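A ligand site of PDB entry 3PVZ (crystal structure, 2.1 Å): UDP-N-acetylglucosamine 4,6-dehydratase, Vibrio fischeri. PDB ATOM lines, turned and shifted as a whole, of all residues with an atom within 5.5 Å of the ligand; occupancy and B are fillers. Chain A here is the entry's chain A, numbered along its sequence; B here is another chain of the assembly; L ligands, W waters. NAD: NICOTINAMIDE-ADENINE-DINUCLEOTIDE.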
ATOM      1  N   GLY A  42      -3.336 -17.073 -19.084  1.00  0.00           N
ATOM      2  CA  GLY A  42      -3.678 -17.432 -20.448  1.00  0.00           C
ATOM      3  C   GLY A  42      -3.519 -18.918 -20.660  1.00  0.00           C
ATOM      4  O   GLY A  42      -3.237 -19.399 -21.792  1.00  0.00           O
ATOM      5  N   GLY A  43      -3.758 -19.649 -19.593  1.00  0.00           N
ATOM      6  CA  GLY A  43      -3.505 -21.078 -19.619  1.00  0.00           C
ATOM      7  C   GLY A  43      -4.534 -21.878 -20.368  1.00  0.00           C
ATOM      8  O   GLY A  43      -4.330 -23.042 -20.500  1.00  0.00           O
ATOM      9  N   ALA A  44      -5.664 -21.299 -20.776  1.00  0.00           N
ATOM     10  CA  ALA A  44      -6.614 -22.001 -21.667  1.00  0.00           C
ATOM     11  C   ALA A  44      -6.295 -21.789 -23.153  1.00  0.00           C
ATOM     12  O   ALA A  44      -6.991 -22.286 -24.019  1.00  0.00           O
ATOM     13  CB  ALA A  44      -8.058 -21.595 -21.397  1.00  0.00           C
ATOM     14  N   GLY A  45      -5.256 -21.035 -23.447  1.00  0.00           N
ATOM     15  CA  GLY A  45      -4.926 -20.686 -24.824  1.00  0.00           C
ATOM     16  C   GLY A  45      -4.097 -21.802 -25.405  1.00  0.00           C
ATOM     17  O   GLY A  45      -3.795 -22.795 -24.730  1.00  0.00           O
ATOM     18  N   SER A  46      -3.676 -21.643 -26.666  1.00  0.00           N
ATOM     19  CA  SER A  46      -2.986 -22.736 -27.342  1.00  0.00           C
ATOM     20  C   SER A  46      -1.642 -23.052 -26.722  1.00  0.00           C
ATOM     21  O   SER A  46      -1.421 -24.209 -26.353  1.00  0.00           O
ATOM     22  CB  SER A  46      -2.863 -22.466 -28.844  1.00  0.00           C
ATOM     23  OG  SER A  46      -4.139 -22.648 -29.447  1.00  0.00           O
ATOM     24  N   ILE A  47      -0.737 -22.090 -26.582  1.00  0.00           N
ATOM     25  CA  ILE A  47       0.504 -22.410 -25.865  1.00  0.00           C
ATOM     26  C   ILE A  47       0.251 -22.620 -24.337  1.00  0.00           C
ATOM     27  O   ILE A  47       0.826 -23.553 -23.704  1.00  0.00           O
ATOM     28  CB  ILE A  47       1.573 -21.371 -26.113  1.00  0.00           C
ATOM     29  CG1 ILE A  47       1.851 -21.273 -27.638  1.00  0.00           C
ATOM     30  CG2 ILE A  47       2.829 -21.837 -25.366  1.00  0.00           C
ATOM     31  CD1 ILE A  47       2.587 -19.995 -28.181  1.00  0.00           C
ATOM     32  N   GLY A  48      -0.680 -21.849 -23.763  1.00  0.00           N
ATOM     33  CA  GLY A  48      -1.040 -21.978 -22.356  1.00  0.00           C
ATOM     34  C   GLY A  48      -1.396 -23.399 -21.964  1.00  0.00           C
ATOM     35  O   GLY A  48      -0.902 -23.927 -21.006  1.00  0.00           O
ATOM     36  N   VAL A  66      -5.402 -19.635 -15.133  1.00  0.00           N
ATOM     37  CA  VAL A  66      -6.313 -18.473 -15.238  1.00  0.00           C
ATOM     38  C   VAL A  66      -6.505 -18.010 -16.677  1.00  0.00           C
ATOM     39  O   VAL A  66      -5.556 -17.812 -17.395  1.00  0.00           O
ATOM     40  CB  VAL A  66      -5.731 -17.330 -14.451  1.00  0.00           C
ATOM     41  CG1 VAL A  66      -6.676 -16.028 -14.536  1.00  0.00           C
ATOM     42  CG2 VAL A  66      -5.567 -17.744 -12.975  1.00  0.00           C
ATOM     43  N   ASP A  67      -7.744 -17.836 -17.127  1.00  0.00           N
ATOM     44  CA  ASP A  67      -7.989 -17.432 -18.513  1.00  0.00           C
ATOM     45  C   ASP A  67      -9.413 -16.953 -18.594  1.00  0.00           C
ATOM     46  O   ASP A  67     -10.266 -17.417 -17.850  1.00  0.00           O
ATOM     47  CB  ASP A  67      -7.817 -18.644 -19.453  1.00  0.00           C
ATOM     48  CG  ASP A  67      -7.658 -18.245 -20.884  1.00  0.00           C
ATOM     49  OD1 ASP A  67      -8.648 -17.781 -21.527  1.00  0.00           O
ATOM     50  OD2 ASP A  67      -6.528 -18.485 -21.385  1.00  0.00           O
ATOM     51  N   ILE A  68      -9.675 -16.049 -19.506  1.00  0.00           N
ATOM     52  CA  ILE A  68     -11.011 -15.513 -19.601  1.00  0.00           C
ATOM     53  C   ILE A  68     -11.941 -16.489 -20.249  1.00  0.00           C
ATOM     54  O   ILE A  68     -13.119 -16.420 -20.001  1.00  0.00           O
ATOM     55  CB  ILE A  68     -11.118 -14.155 -20.344  1.00  0.00           C
ATOM     56  CG1 ILE A  68     -10.336 -14.176 -21.640  1.00  0.00           C
ATOM     57  CG2 ILE A  68     -10.604 -13.044 -19.500  1.00  0.00           C
ATOM     58  CD1 ILE A  68     -10.542 -12.941 -22.465  1.00  0.00           C
ATOM     59  N   SER A  69     -11.429 -17.451 -21.028  1.00  0.00           N
ATOM     60  CA  SER A  69     -12.313 -18.381 -21.706  1.00  0.00           C
ATOM     61  C   SER A  69     -12.730 -19.538 -20.782  1.00  0.00           C
ATOM     62  O   SER A  69     -11.948 -20.448 -20.555  1.00  0.00           O
ATOM     63  CB  SER A  69     -11.652 -18.927 -22.996  1.00  0.00           C
ATOM     64  OG  SER A  69     -12.411 -19.999 -23.532  1.00  0.00           O
ATOM     65  N   ASN A  72     -12.880 -22.835 -23.165  1.00  0.00           N
ATOM     66  CA  ASN A  72     -11.603 -23.514 -23.417  1.00  0.00           C
ATOM     67  C   ASN A  72     -10.982 -24.103 -22.157  1.00  0.00           C
ATOM     68  O   ASN A  72     -10.316 -25.141 -22.175  1.00  0.00           O
ATOM     69  CB  ASN A  72     -10.642 -22.570 -24.170  1.00  0.00           C
ATOM     70  CG  ASN A  72     -11.174 -22.250 -25.539  1.00  0.00           C
ATOM     71  OD1 ASN A  72     -11.905 -23.057 -26.088  1.00  0.00           O
ATOM     72  ND2 ASN A  72     -10.879 -21.094 -26.064  1.00  0.00           N
ATOM     73  N   LEU A  96     -10.837 -15.966 -15.041  1.00  0.00           N
ATOM     74  CA  LEU A  96     -10.711 -14.583 -14.669  1.00  0.00           C
ATOM     75  C   LEU A  96      -9.940 -13.808 -15.766  1.00  0.00           C
ATOM     76  O   LEU A  96      -9.134 -14.367 -16.510  1.00  0.00           O
ATOM     77  CB  LEU A  96      -9.955 -14.492 -13.360  1.00  0.00           C
ATOM     78  CG  LEU A  96     -10.493 -15.117 -12.069  1.00  0.00           C
ATOM     79  CD1 LEU A  96      -9.459 -14.907 -10.883  1.00  0.00           C
ATOM     80  CD2 LEU A  96     -11.811 -14.545 -11.761  1.00  0.00           C
ATOM     81  N   ASP A  97     -10.288 -12.535 -15.905  1.00  0.00           N
ATOM     82  CA  ASP A  97      -9.596 -11.606 -16.706  1.00  0.00           C
ATOM     83  C   ASP A  97      -8.515 -10.969 -15.820  1.00  0.00           C
ATOM     84  O   ASP A  97      -8.814 -10.416 -14.742  1.00  0.00           O
ATOM     85  CB  ASP A  97     -10.584 -10.537 -17.134  1.00  0.00           C
ATOM     86  CG  ASP A  97      -9.966  -9.512 -18.090  1.00  0.00           C
ATOM     87  OD1 ASP A  97      -8.817  -9.025 -17.845  1.00  0.00           O
ATOM     88  OD2 ASP A  97     -10.659  -9.184 -19.090  1.00  0.00           O
ATOM     89  N   ILE A  98      -7.289 -11.005 -16.277  1.00  0.00           N
ATOM     90  CA  ILE A  98      -6.135 -10.586 -15.467  1.00  0.00           C
ATOM     91  C   ILE A  98      -6.192  -9.067 -15.123  1.00  0.00           C
ATOM     92  O   ILE A  98      -5.607  -8.628 -14.110  1.00  0.00           O
ATOM     93  CB  ILE A  98      -4.869 -10.923 -16.235  1.00  0.00           C
ATOM     94  CG1 ILE A  98      -4.703 -12.436 -16.320  1.00  0.00           C
ATOM     95  CG2 ILE A  98      -3.615 -10.293 -15.616  1.00  0.00           C
ATOM     96  CD1 ILE A  98      -3.703 -12.823 -17.450  1.00  0.00           C
ATOM     97  N   GLY A  99      -6.852  -8.283 -15.957  1.00  0.00           N
ATOM     98  CA  GLY A  99      -7.039  -6.854 -15.709  1.00  0.00           C
ATOM     99  C   GLY A  99      -8.071  -6.468 -14.653  1.00  0.00           C
ATOM    100  O   GLY A  99      -8.271  -5.304 -14.396  1.00  0.00           O
ATOM    101  N   LEU A 119       1.026 -16.644 -20.741  1.00  0.00           N
ATOM    102  CA  LEU A 119       0.820 -16.949 -22.133  1.00  0.00           C
ATOM    103  C   LEU A 119      -0.461 -16.258 -22.566  1.00  0.00           C
ATOM    104  O   LEU A 119      -1.088 -16.668 -23.516  1.00  0.00           O
ATOM    105  CB  LEU A 119       0.676 -18.481 -22.368  1.00  0.00           C
ATOM    106  CG  LEU A 119       1.958 -19.308 -22.280  1.00  0.00           C
ATOM    107  CD1 LEU A 119       3.060 -18.730 -23.190  1.00  0.00           C
ATOM    108  CD2 LEU A 119       2.430 -19.457 -20.825  1.00  0.00           C
ATOM    109  N   SER A 120      -0.833 -15.169 -21.898  1.00  0.00           N
ATOM    110  CA  SER A 120      -2.036 -14.432 -22.288  1.00  0.00           C
ATOM    111  C   SER A 120      -1.606 -13.304 -23.224  1.00  0.00           C
ATOM    112  O   SER A 120      -0.505 -12.793 -23.093  1.00  0.00           O
ATOM    113  CB  SER A 120      -2.765 -13.904 -21.048  1.00  0.00           C
ATOM    114  OG  SER A 120      -2.116 -12.731 -20.550  1.00  0.00           O
ATOM    115  N   ALA A 121      -2.496 -12.918 -24.125  1.00  0.00           N
ATOM    116  CA  ALA A 121      -2.212 -11.882 -25.163  1.00  0.00           C
ATOM    117  C   ALA A 121      -3.416 -11.639 -26.011  1.00  0.00           C
ATOM    118  O   ALA A 121      -4.330 -12.467 -26.056  1.00  0.00           O
ATOM    119  CB  ALA A 121      -1.090 -12.288 -26.110  1.00  0.00           C
ATOM    120  N   LEU A 122      -3.379 -10.490 -26.684  1.00  0.00           N
ATOM    121  CA  LEU A 122      -4.061 -10.292 -27.950  1.00  0.00           C
ATOM    122  C   LEU A 122      -2.986 -10.382 -29.008  1.00  0.00           C
ATOM    123  O   LEU A 122      -1.969  -9.688 -28.888  1.00  0.00           O
ATOM    124  CB  LEU A 122      -4.739  -8.914 -28.045  1.00  0.00           C
ATOM    125  CG  LEU A 122      -6.231  -8.961 -27.779  1.00  0.00           C
ATOM    126  CD1 LEU A 122      -6.430  -9.080 -26.246  1.00  0.00           C
ATOM    127  CD2 LEU A 122      -6.903  -7.712 -28.338  1.00  0.00           C
ATOM    128  N   LYS A 123      -3.202 -11.252 -30.003  1.00  0.00           N
ATOM    129  CA  LYS A 123      -2.133 -11.598 -30.938  1.00  0.00           C
ATOM    130  C   LYS A 123      -2.447 -11.356 -32.413  1.00  0.00           C
ATOM    131  O   LYS A 123      -1.518 -11.407 -33.205  1.00  0.00           O
ATOM    132  CB  LYS A 123      -1.695 -13.073 -30.756  1.00  0.00           C
ATOM    133  CG  LYS A 123      -2.792 -14.107 -31.155  1.00  0.00           C
ATOM    134  CD  LYS A 123      -2.238 -15.497 -31.367  1.00  0.00           C
ATOM    135  CE  LYS A 123      -3.384 -16.493 -31.658  1.00  0.00           C
ATOM    136  NZ  LYS A 123      -2.852 -17.920 -31.764  1.00  0.00           N
ATOM    137  N   ARG A 136      -7.040  -2.145 -25.990  1.00  0.00           N
ATOM    138  CA  ARG A 136      -7.127  -3.372 -25.239  1.00  0.00           C
ATOM    139  C   ARG A 136      -5.855  -4.228 -25.367  1.00  0.00           C
ATOM    140  O   ARG A 136      -5.446  -4.874 -24.444  1.00  0.00           O
ATOM    141  CB  ARG A 136      -8.376  -4.193 -25.641  1.00  0.00           C
ATOM    142  CG  ARG A 136      -8.435  -5.487 -24.861  1.00  0.00           C
ATOM    143  CD  ARG A 136      -9.654  -6.325 -25.133  1.00  0.00           C
ATOM    144  NE  ARG A 136      -9.504  -7.580 -24.415  1.00  0.00           N
ATOM    145  CZ  ARG A 136      -9.824  -8.789 -24.879  1.00  0.00           C
ATOM    146  NH1 ARG A 136     -10.313  -8.954 -26.098  1.00  0.00           N
ATOM    147  NH2 ARG A 136      -9.586  -9.851 -24.166  1.00  0.00           N
ATOM    148  N   VAL A 140      -3.727  -5.611 -22.342  1.00  0.00           N
ATOM    149  CA  VAL A 140      -3.439  -7.047 -22.199  1.00  0.00           C
ATOM    150  C   VAL A 140      -1.949  -7.353 -22.419  1.00  0.00           C
ATOM    151  O   VAL A 140      -1.374  -8.121 -21.654  1.00  0.00           O
ATOM    152  CB  VAL A 140      -4.265  -7.903 -23.135  1.00  0.00           C
ATOM    153  CG1 VAL A 140      -3.782  -9.374 -23.063  1.00  0.00           C
ATOM    154  CG2 VAL A 140      -5.759  -7.812 -22.819  1.00  0.00           C
ATOM    155  N   ASN A 144      -1.038  -5.469 -18.212  1.00  0.00           N
ATOM    156  CA  ASN A 144      -1.333  -6.673 -17.449  1.00  0.00           C
ATOM    157  C   ASN A 144      -0.047  -7.415 -17.149  1.00  0.00           C
ATOM    158  O   ASN A 144       0.103  -8.071 -16.088  1.00  0.00           O
ATOM    159  CB  ASN A 144      -2.253  -7.621 -18.220  1.00  0.00           C
ATOM    160  CG  ASN A 144      -3.711  -7.150 -18.247  1.00  0.00           C
ATOM    161  OD1 ASN A 144      -4.064  -6.096 -17.709  1.00  0.00           O
ATOM    162  ND2 ASN A 144      -4.560  -7.940 -18.898  1.00  0.00           N
ATOM    163  N   VAL A 163       6.304 -14.510 -23.199  1.00  0.00           N
ATOM    164  CA  VAL A 163       6.723 -14.672 -24.586  1.00  0.00           C
ATOM    165  C   VAL A 163       7.499 -13.473 -25.071  1.00  0.00           C
ATOM    166  O   VAL A 163       7.243 -12.359 -24.633  1.00  0.00           O
ATOM    167  CB  VAL A 163       5.535 -14.832 -25.526  1.00  0.00           C
ATOM    168  CG1 VAL A 163       4.577 -15.868 -24.987  1.00  0.00           C
ATOM    169  CG2 VAL A 163       4.853 -13.461 -25.724  1.00  0.00           C
ATOM    170  N   SER A 164       8.425 -13.704 -26.003  1.00  0.00           N
ATOM    171  CA  SER A 164       9.114 -12.626 -26.691  1.00  0.00           C
ATOM    172  C   SER A 164       8.423 -12.275 -27.990  1.00  0.00           C
ATOM    173  O   SER A 164       7.576 -13.047 -28.474  1.00  0.00           O
ATOM    174  CB  SER A 164      10.559 -13.012 -26.973  1.00  0.00           C
ATOM    175  OG  SER A 164      11.394 -12.555 -25.948  1.00  0.00           O
ATOM    176  N   ASP A 166       8.031 -12.183 -31.852  1.00  0.00           N
ATOM    177  CA  ASP A 166       8.234 -13.340 -32.755  1.00  0.00           C
ATOM    178  C   ASP A 166       9.586 -13.281 -33.484  1.00  0.00           C
ATOM    179  O   ASP A 166      10.152 -14.329 -33.828  1.00  0.00           O
ATOM    180  CB  ASP A 166       7.116 -13.421 -33.799  1.00  0.00           C
ATOM    181  CG  ASP A 166       5.750 -13.676 -33.205  1.00  0.00           C
ATOM    182  OD1 ASP A 166       5.603 -13.823 -31.971  1.00  0.00           O
ATOM    183  OD2 ASP A 166       4.783 -13.703 -33.987  1.00  0.00           O
ATOM    184  N   MET A 175       1.008  -4.732 -33.242  1.00  0.00           N
ATOM    185  CA  MET A 175       1.181  -5.961 -32.471  1.00  0.00           C
ATOM    186  C   MET A 175       2.609  -6.127 -31.988  1.00  0.00           C
ATOM    187  O   MET A 175       2.875  -6.243 -30.785  1.00  0.00           O
ATOM    188  CB  MET A 175       0.869  -7.168 -33.359  1.00  0.00           C
ATOM    189  CG  MET A 175      -0.315  -7.890 -33.000  1.00  0.00           C
ATOM    190  SD  MET A 175       0.069  -8.724 -31.322  1.00  0.00           S
ATOM    191  CE  MET A 175       1.473  -9.899 -32.052  1.00  0.00           C
ATOM    192  N   LYS A 179       4.411  -5.788 -28.277  1.00  0.00           N
ATOM    193  CA  LYS A 179       5.323  -6.767 -27.653  1.00  0.00           C
ATOM    194  C   LYS A 179       6.720  -6.137 -27.460  1.00  0.00           C
ATOM    195  O   LYS A 179       7.434  -6.459 -26.509  1.00  0.00           O
ATOM    196  CB  LYS A 179       5.435  -8.069 -28.458  1.00  0.00           C
ATOM    197  CG  LYS A 179       4.107  -8.829 -28.788  1.00  0.00           C
ATOM    198  CD  LYS A 179       3.650  -9.725 -27.633  1.00  0.00           C
ATOM    199  CE  LYS A 179       2.545 -10.741 -28.073  1.00  0.00           C
ATOM    200  NZ  LYS A 179       3.092 -11.923 -28.799  1.00  0.00           N
ATOM    201  N   PHE A 200       8.861 -18.260 -30.543  1.00  0.00           N
ATOM    202  CA  PHE A 200       8.295 -19.450 -31.204  1.00  0.00           C
ATOM    203  C   PHE A 200       8.200 -19.310 -32.739  1.00  0.00           C
ATOM    204  O   PHE A 200       8.058 -18.211 -33.244  1.00  0.00           O
ATOM    205  CB  PHE A 200       6.872 -19.724 -30.716  1.00  0.00           C
ATOM    206  CG  PHE A 200       6.732 -19.918 -29.226  1.00  0.00           C
ATOM    207  CD1 PHE A 200       6.820 -21.160 -28.647  1.00  0.00           C
ATOM    208  CD2 PHE A 200       6.405 -18.844 -28.423  1.00  0.00           C
ATOM    209  CE1 PHE A 200       6.605 -21.328 -27.283  1.00  0.00           C
ATOM    210  CE2 PHE A 200       6.236 -19.021 -27.063  1.00  0.00           C
ATOM    211  CZ  PHE A 200       6.364 -20.260 -26.497  1.00  0.00           C
ATOM    212  N   ALA A 201       8.351 -20.430 -33.427  1.00  0.00           N
ATOM    213  CA  ALA A 201       7.871 -20.653 -34.791  1.00  0.00           C
ATOM    214  C   ALA A 201       6.336 -20.679 -34.787  1.00  0.00           C
ATOM    215  O   ALA A 201       5.710 -20.566 -33.741  1.00  0.00           O
ATOM    216  CB  ALA A 201       8.391 -22.008 -35.281  1.00  0.00           C
ATOM    217  N   ASN A 202       5.725 -20.879 -35.932  1.00  0.00           N
ATOM    218  CA  ASN A 202       4.282 -21.089 -35.940  1.00  0.00           C
ATOM    219  C   ASN A 202       3.878 -22.358 -35.230  1.00  0.00           C
ATOM    220  O   ASN A 202       4.343 -23.438 -35.592  1.00  0.00           O
ATOM    221  CB  ASN A 202       3.778 -21.154 -37.364  1.00  0.00           C
ATOM    222  CG  ASN A 202       3.762 -19.819 -38.039  1.00  0.00           C
ATOM    223  OD1 ASN A 202       4.706 -19.063 -37.944  1.00  0.00           O
ATOM    224  ND2 ASN A 202       2.688 -19.530 -38.733  1.00  0.00           N
ATOM    225  N   VAL A 203       2.978 -22.263 -34.251  1.00  0.00           N
ATOM    226  CA  VAL A 203       2.543 -23.433 -33.520  1.00  0.00           C
ATOM    227  C   VAL A 203       1.350 -24.126 -34.217  1.00  0.00           C
ATOM    228  O   VAL A 203       0.235 -23.605 -34.234  1.00  0.00           O
ATOM    229  CB  VAL A 203       2.218 -23.092 -32.055  1.00  0.00           C
ATOM    230  CG1 VAL A 203       1.810 -24.373 -31.311  1.00  0.00           C
ATOM    231  CG2 VAL A 203       3.431 -22.440 -31.351  1.00  0.00           C
ATOM    232  N   SER A 206      -2.611 -23.904 -33.673  1.00  0.00           N
ATOM    233  CA  SER A 206      -2.951 -23.018 -32.573  1.00  0.00           C
ATOM    234  C   SER A 206      -4.253 -22.267 -32.921  1.00  0.00           C
ATOM    235  O   SER A 206      -4.569 -21.999 -34.101  1.00  0.00           O
ATOM    236  CB  SER A 206      -1.806 -22.083 -32.233  1.00  0.00           C
ATOM    237  OG  SER A 206      -1.558 -21.157 -33.249  1.00  0.00           O
ATOM    238  N   ASP A 207      -5.042 -22.030 -31.886  1.00  0.00           N
ATOM    239  CA  ASP A 207      -6.317 -21.331 -31.985  1.00  0.00           C
ATOM    240  C   ASP A 207      -6.197 -20.030 -32.754  1.00  0.00           C
ATOM    241  O   ASP A 207      -5.244 -19.288 -32.565  1.00  0.00           O
ATOM    242  CB  ASP A 207      -6.871 -21.037 -30.567  1.00  0.00           C
ATOM    243  CG  ASP A 207      -8.384 -20.796 -30.544  1.00  0.00           C
ATOM    244  OD1 ASP A 207      -9.068 -21.018 -31.578  1.00  0.00           O
ATOM    245  OD2 ASP A 207      -8.921 -20.408 -29.458  1.00  0.00           O
ATOM    246  N   GLU B  70     -11.043 -12.789 -28.937  1.00  0.00           N
ATOM    247  CA  GLU B  70     -10.391 -12.405 -30.168  1.00  0.00           C
ATOM    248  C   GLU B  70     -10.398 -13.590 -31.169  1.00  0.00           C
ATOM    249  O   GLU B  70     -10.814 -13.429 -32.317  1.00  0.00           O
ATOM    250  CB  GLU B  70      -8.951 -11.967 -29.823  1.00  0.00           C
ATOM    251  CG  GLU B  70      -8.148 -11.464 -30.977  1.00  0.00           C
ATOM    252  CD  GLU B  70      -6.657 -11.387 -30.676  1.00  0.00           C
ATOM    253  OE1 GLU B  70      -6.053 -10.362 -31.067  1.00  0.00           O
ATOM    254  OE2 GLU B  70      -6.076 -12.339 -30.116  1.00  0.00           O
ATOM    255  N   ASN B  71      -9.998 -14.780 -30.717  1.00  0.00           N
ATOM    256  CA  ASN B  71      -9.989 -15.948 -31.598  1.00  0.00           C
ATOM    257  C   ASN B  71     -11.365 -16.344 -32.169  1.00  0.00           C
ATOM    258  O   ASN B  71     -11.499 -16.543 -33.362  1.00  0.00           O
ATOM    259  CB  ASN B  71      -9.357 -17.157 -30.903  1.00  0.00           C
ATOM    260  CG  ASN B  71      -7.859 -17.049 -30.797  1.00  0.00           C
ATOM    261  OD1 ASN B  71      -7.200 -16.388 -31.604  1.00  0.00           O
ATOM    262  ND2 ASN B  71      -7.300 -17.697 -29.806  1.00  0.00           N
HETATM  263  PA  NAD L   1      -4.054 -17.792 -27.861  1.00  0.00           P
HETATM  264  O1A NAD L   1      -5.011 -16.833 -28.489  1.00  0.00           O
HETATM  265  O2A NAD L   1      -4.468 -19.199 -28.159  1.00  0.00           O
HETATM  266  O5B NAD L   1      -4.208 -17.811 -26.278  1.00  0.00           O
HETATM  267  C5B NAD L   1      -4.096 -16.538 -25.616  1.00  0.00           C
HETATM  268  C4B NAD L   1      -4.852 -16.770 -24.303  1.00  0.00           C
HETATM  269  O4B NAD L   1      -4.844 -15.632 -23.467  1.00  0.00           O
HETATM  270  C3B NAD L   1      -6.346 -17.111 -24.609  1.00  0.00           C
HETATM  271  O3B NAD L   1      -6.733 -18.311 -23.965  1.00  0.00           O
HETATM  272  C2B NAD L   1      -7.092 -15.881 -24.044  1.00  0.00           C
HETATM  273  O2B NAD L   1      -8.438 -16.133 -23.657  1.00  0.00           O
HETATM  274  C1B NAD L   1      -6.119 -15.530 -22.895  1.00  0.00           C
HETATM  275  N9A NAD L   1      -6.310 -14.160 -22.450  1.00  0.00           N
HETATM  276  C8A NAD L   1      -6.274 -13.052 -23.204  1.00  0.00           C
HETATM  277  N7A NAD L   1      -6.535 -12.000 -22.505  1.00  0.00           N
HETATM  278  C5A NAD L   1      -6.670 -12.412 -21.206  1.00  0.00           C
HETATM  279  C6A NAD L   1      -6.960 -11.772 -20.014  1.00  0.00           C
HETATM  280  N6A NAD L   1      -7.075 -10.404 -20.037  1.00  0.00           N
HETATM  281  N1A NAD L   1      -7.075 -12.472 -18.884  1.00  0.00           N
HETATM  282  C2A NAD L   1      -6.947 -13.799 -18.901  1.00  0.00           C
HETATM  283  N3A NAD L   1      -6.698 -14.445 -20.016  1.00  0.00           N
HETATM  284  C4A NAD L   1      -6.547 -13.793 -21.163  1.00  0.00           C
HETATM  285  O3  NAD L   1      -2.565 -17.417 -28.327  1.00  0.00           O
HETATM  286  PN  NAD L   1      -1.416 -18.570 -28.333  1.00  0.00           P
HETATM  287  O1N NAD L   1      -1.290 -19.175 -29.719  1.00  0.00           O
HETATM  288  O2N NAD L   1      -1.434 -19.614 -27.285  1.00  0.00           O
HETATM  289  O5D NAD L   1      -0.081 -17.605 -28.269  1.00  0.00           O
HETATM  290  C5D NAD L   1       0.179 -17.158 -26.951  1.00  0.00           C
HETATM  291  C4D NAD L   1       1.396 -16.232 -26.961  1.00  0.00           C
HETATM  292  O4D NAD L   1       2.440 -16.781 -27.816  1.00  0.00           O
HETATM  293  C3D NAD L   1       1.008 -14.867 -27.603  1.00  0.00           C
HETATM  294  O3D NAD L   1       1.813 -13.778 -27.105  1.00  0.00           O
HETATM  295  C2D NAD L   1       1.416 -15.065 -29.077  1.00  0.00           C
HETATM  296  O2D NAD L   1       1.681 -13.814 -29.740  1.00  0.00           O
HETATM  297  C1D NAD L   1       2.702 -15.874 -28.929  1.00  0.00           C
HETATM  298  N1N NAD L   1       3.067 -16.587 -30.160  1.00  0.00           N
HETATM  299  C2N NAD L   1       2.210 -17.495 -30.638  1.00  0.00           C
HETATM  300  C3N NAD L   1       2.507 -18.217 -31.782  1.00  0.00           C
HETATM  301  C7N NAD L   1       1.563 -19.203 -32.340  1.00  0.00           C
HETATM  302  O7N NAD L   1       1.884 -19.718 -33.408  1.00  0.00           O
HETATM  303  N7N NAD L   1       0.396 -19.503 -31.764  1.00  0.00           N
HETATM  304  C4N NAD L   1       3.723 -17.975 -32.453  1.00  0.00           C
HETATM  305  C5N NAD L   1       4.595 -17.033 -31.920  1.00  0.00           C
HETATM  306  C6N NAD L   1       4.236 -16.338 -30.764  1.00  0.00           C
HETATM  307  O   HOH W   1       1.882 -14.375 -32.622  1.00  0.00           O
HETATM  308  O   HOH W   2      -7.423  -7.187 -19.332  1.00  0.00           O
HETATM  309  O   HOH W   3      -1.872 -19.340 -24.510  1.00  0.00           O
HETATM  310  O   HOH W   4      -6.631 -12.981 -26.674  1.00  0.00           O
HETATM  311  O   HOH W   5      -6.487 -14.577 -28.644  1.00  0.00           O
HETATM  312  O   HOH W   6       0.134 -19.916 -35.376  1.00  0.00           O
HETATM  313  O   HOH W   7     -10.067 -14.629 -25.262  1.00  0.00           O
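The side-chain amino group of Lys 179 is in hydrogen-bond range of an oxygen (O2D) of the ligand.
The side-chain carboxylate (OD2) of Asp 67 is in hydrogen-bond range of an oxygen (O3B) of the ligand, 2.6 Å away.
The backbone NH (N) of Ile 47 sits at hydrogen-bond distance from an oxygen (O2N) of the ligand, 2.7 Å away.
The side-chain amide nitrogen of Asn 71 of chain B lies within hydrogen-bond range of an oxygen (O1A) of the ligand (2.8 Å).
An oxygen (O1N) of the ligand lies within salt-bridge range of the side-chain amino group (NZ) of Lys 123, 2.9 Å away.
N of Val 203 lies within hydrogen-bond range of O7N of the ligand (2.9 Å).
A nitrogen (N7N) of the ligand sits at hydrogen-bond distance from the side-chain hydroxyl (OG) of Ser 206 (3.0 Å).
The backbone NH of Ser 46 lies within hydrogen-bond range of an oxygen (O2A) of the ligand (3.0 Å).
N of Ile 98 lies within hydrogen-bond range of N1A of the ligand.
An oxygen (O3B) of the ligand lies close to the backbone NH (N) of Gly 45.
The side-chain carboxylate (OD1) of Asp 97 lies within hydrogen-bond range of a nitrogen (N6A) of the ligand (3.1 Å).
A nitrogen (N3A) of the ligand lies within hydrogen-bond range of the backbone NH of Ile 68, 3.4 Å away.
The backbone carbonyl oxygen (O) of Asp 67 is in hydrogen-bond range of the backbone NH (N) of Leu 96 (3.2 Å).
The side-chain carboxylate (OD1) of Asp 67 is in hydrogen-bond range of the backbone NH (N) of Ser 69 (2.8 Å).
The side-chain amide nitrogen of Asn 71 of chain B lies within hydrogen-bond range of the side-chain carboxylate of Asp 207, 3.2 Å away.
O of Asp 207 sits at hydrogen-bond distance from NZ of Lys 123, 2.9 Å away.
The side-chain carboxylate (OE2) of Glu 70 of chain B is in hydrogen-bond range of the backbone NH (N) of Lys 123, 3.1 Å away.
O of Val 203 is in hydrogen-bond range of OG of Ser 206 (3.2 Å).
The side-chain carboxylate (OD1) of Asp 97 sits at hydrogen-bond distance from the backbone NH (N) of Gly 99 (2.8 Å).
The backbone NH (N) of Ile 68 sits at hydrogen-bond distance from the backbone carbonyl oxygen (O) of Leu 96 (3.5 Å).
Residues that only touch the ligand: Asp 166 (3.1 Å), Ser 120 (3.3 Å), Leu 96 (3.3 Å), Val 163 (3.4 Å), Ala 121 (3.4 Å), Ala 201 (3.5 Å), Ala 44 (3.6 Å), Leu 119 (3.7 Å), Asn 144 (3.7 Å), Gly 42 (3.7 Å), Phe 200 (3.7 Å), Asn 202 (3.7 Å), Val 140 (3.8 Å) and Asp 207 (3.9 Å).
Hydrophobic or aromatic side chains that line the ligand: Ile 47, Ile 68, Ile 98, Ala 121, Val 140, Val 163, Phe 200 and Val 203.
Along chain A the residues within 4 Å of the ligand span positions 42 to 207.
The nearest printed residue that does not touch the ligand is Arg 136 (4.1 Å).
Water W6 lies within hydrogen-bond range of an oxygen (O7N) of the ligand (2.6 Å) and the side-chain hydroxyl (OG) of Ser 206 (3.0 Å).
Water W5 lies within hydrogen-bond range of an oxygen (O1A) of the ligand, the side-chain carboxylate (OE2) of Glu 70 of chain B and the side-chain amide nitrogen (ND2) of Asn 71 of chain B.
Water W3 lies within hydrogen-bond range of an oxygen (O2N) of the ligand (2.8 Å), the backbone NH (N) of Gly 48 (2.9 Å), the backbone carbonyl oxygen (O) of Leu 119 (3.0 Å) and the backbone carbonyl oxygen (O) of Gly 42 (3.0 Å).
Water W1 bridges an oxygen (O2D) of the ligand (2.9 Å) and the side-chain carboxylate (OD2) of Asp 166 (3.3 Å).
Water W2 lies within hydrogen-bond range of OD1 of Asp 97 (2.7 Å), ND2 of Asn 144 (3.0 Å) and N6A of the ligand (3.3 Å).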
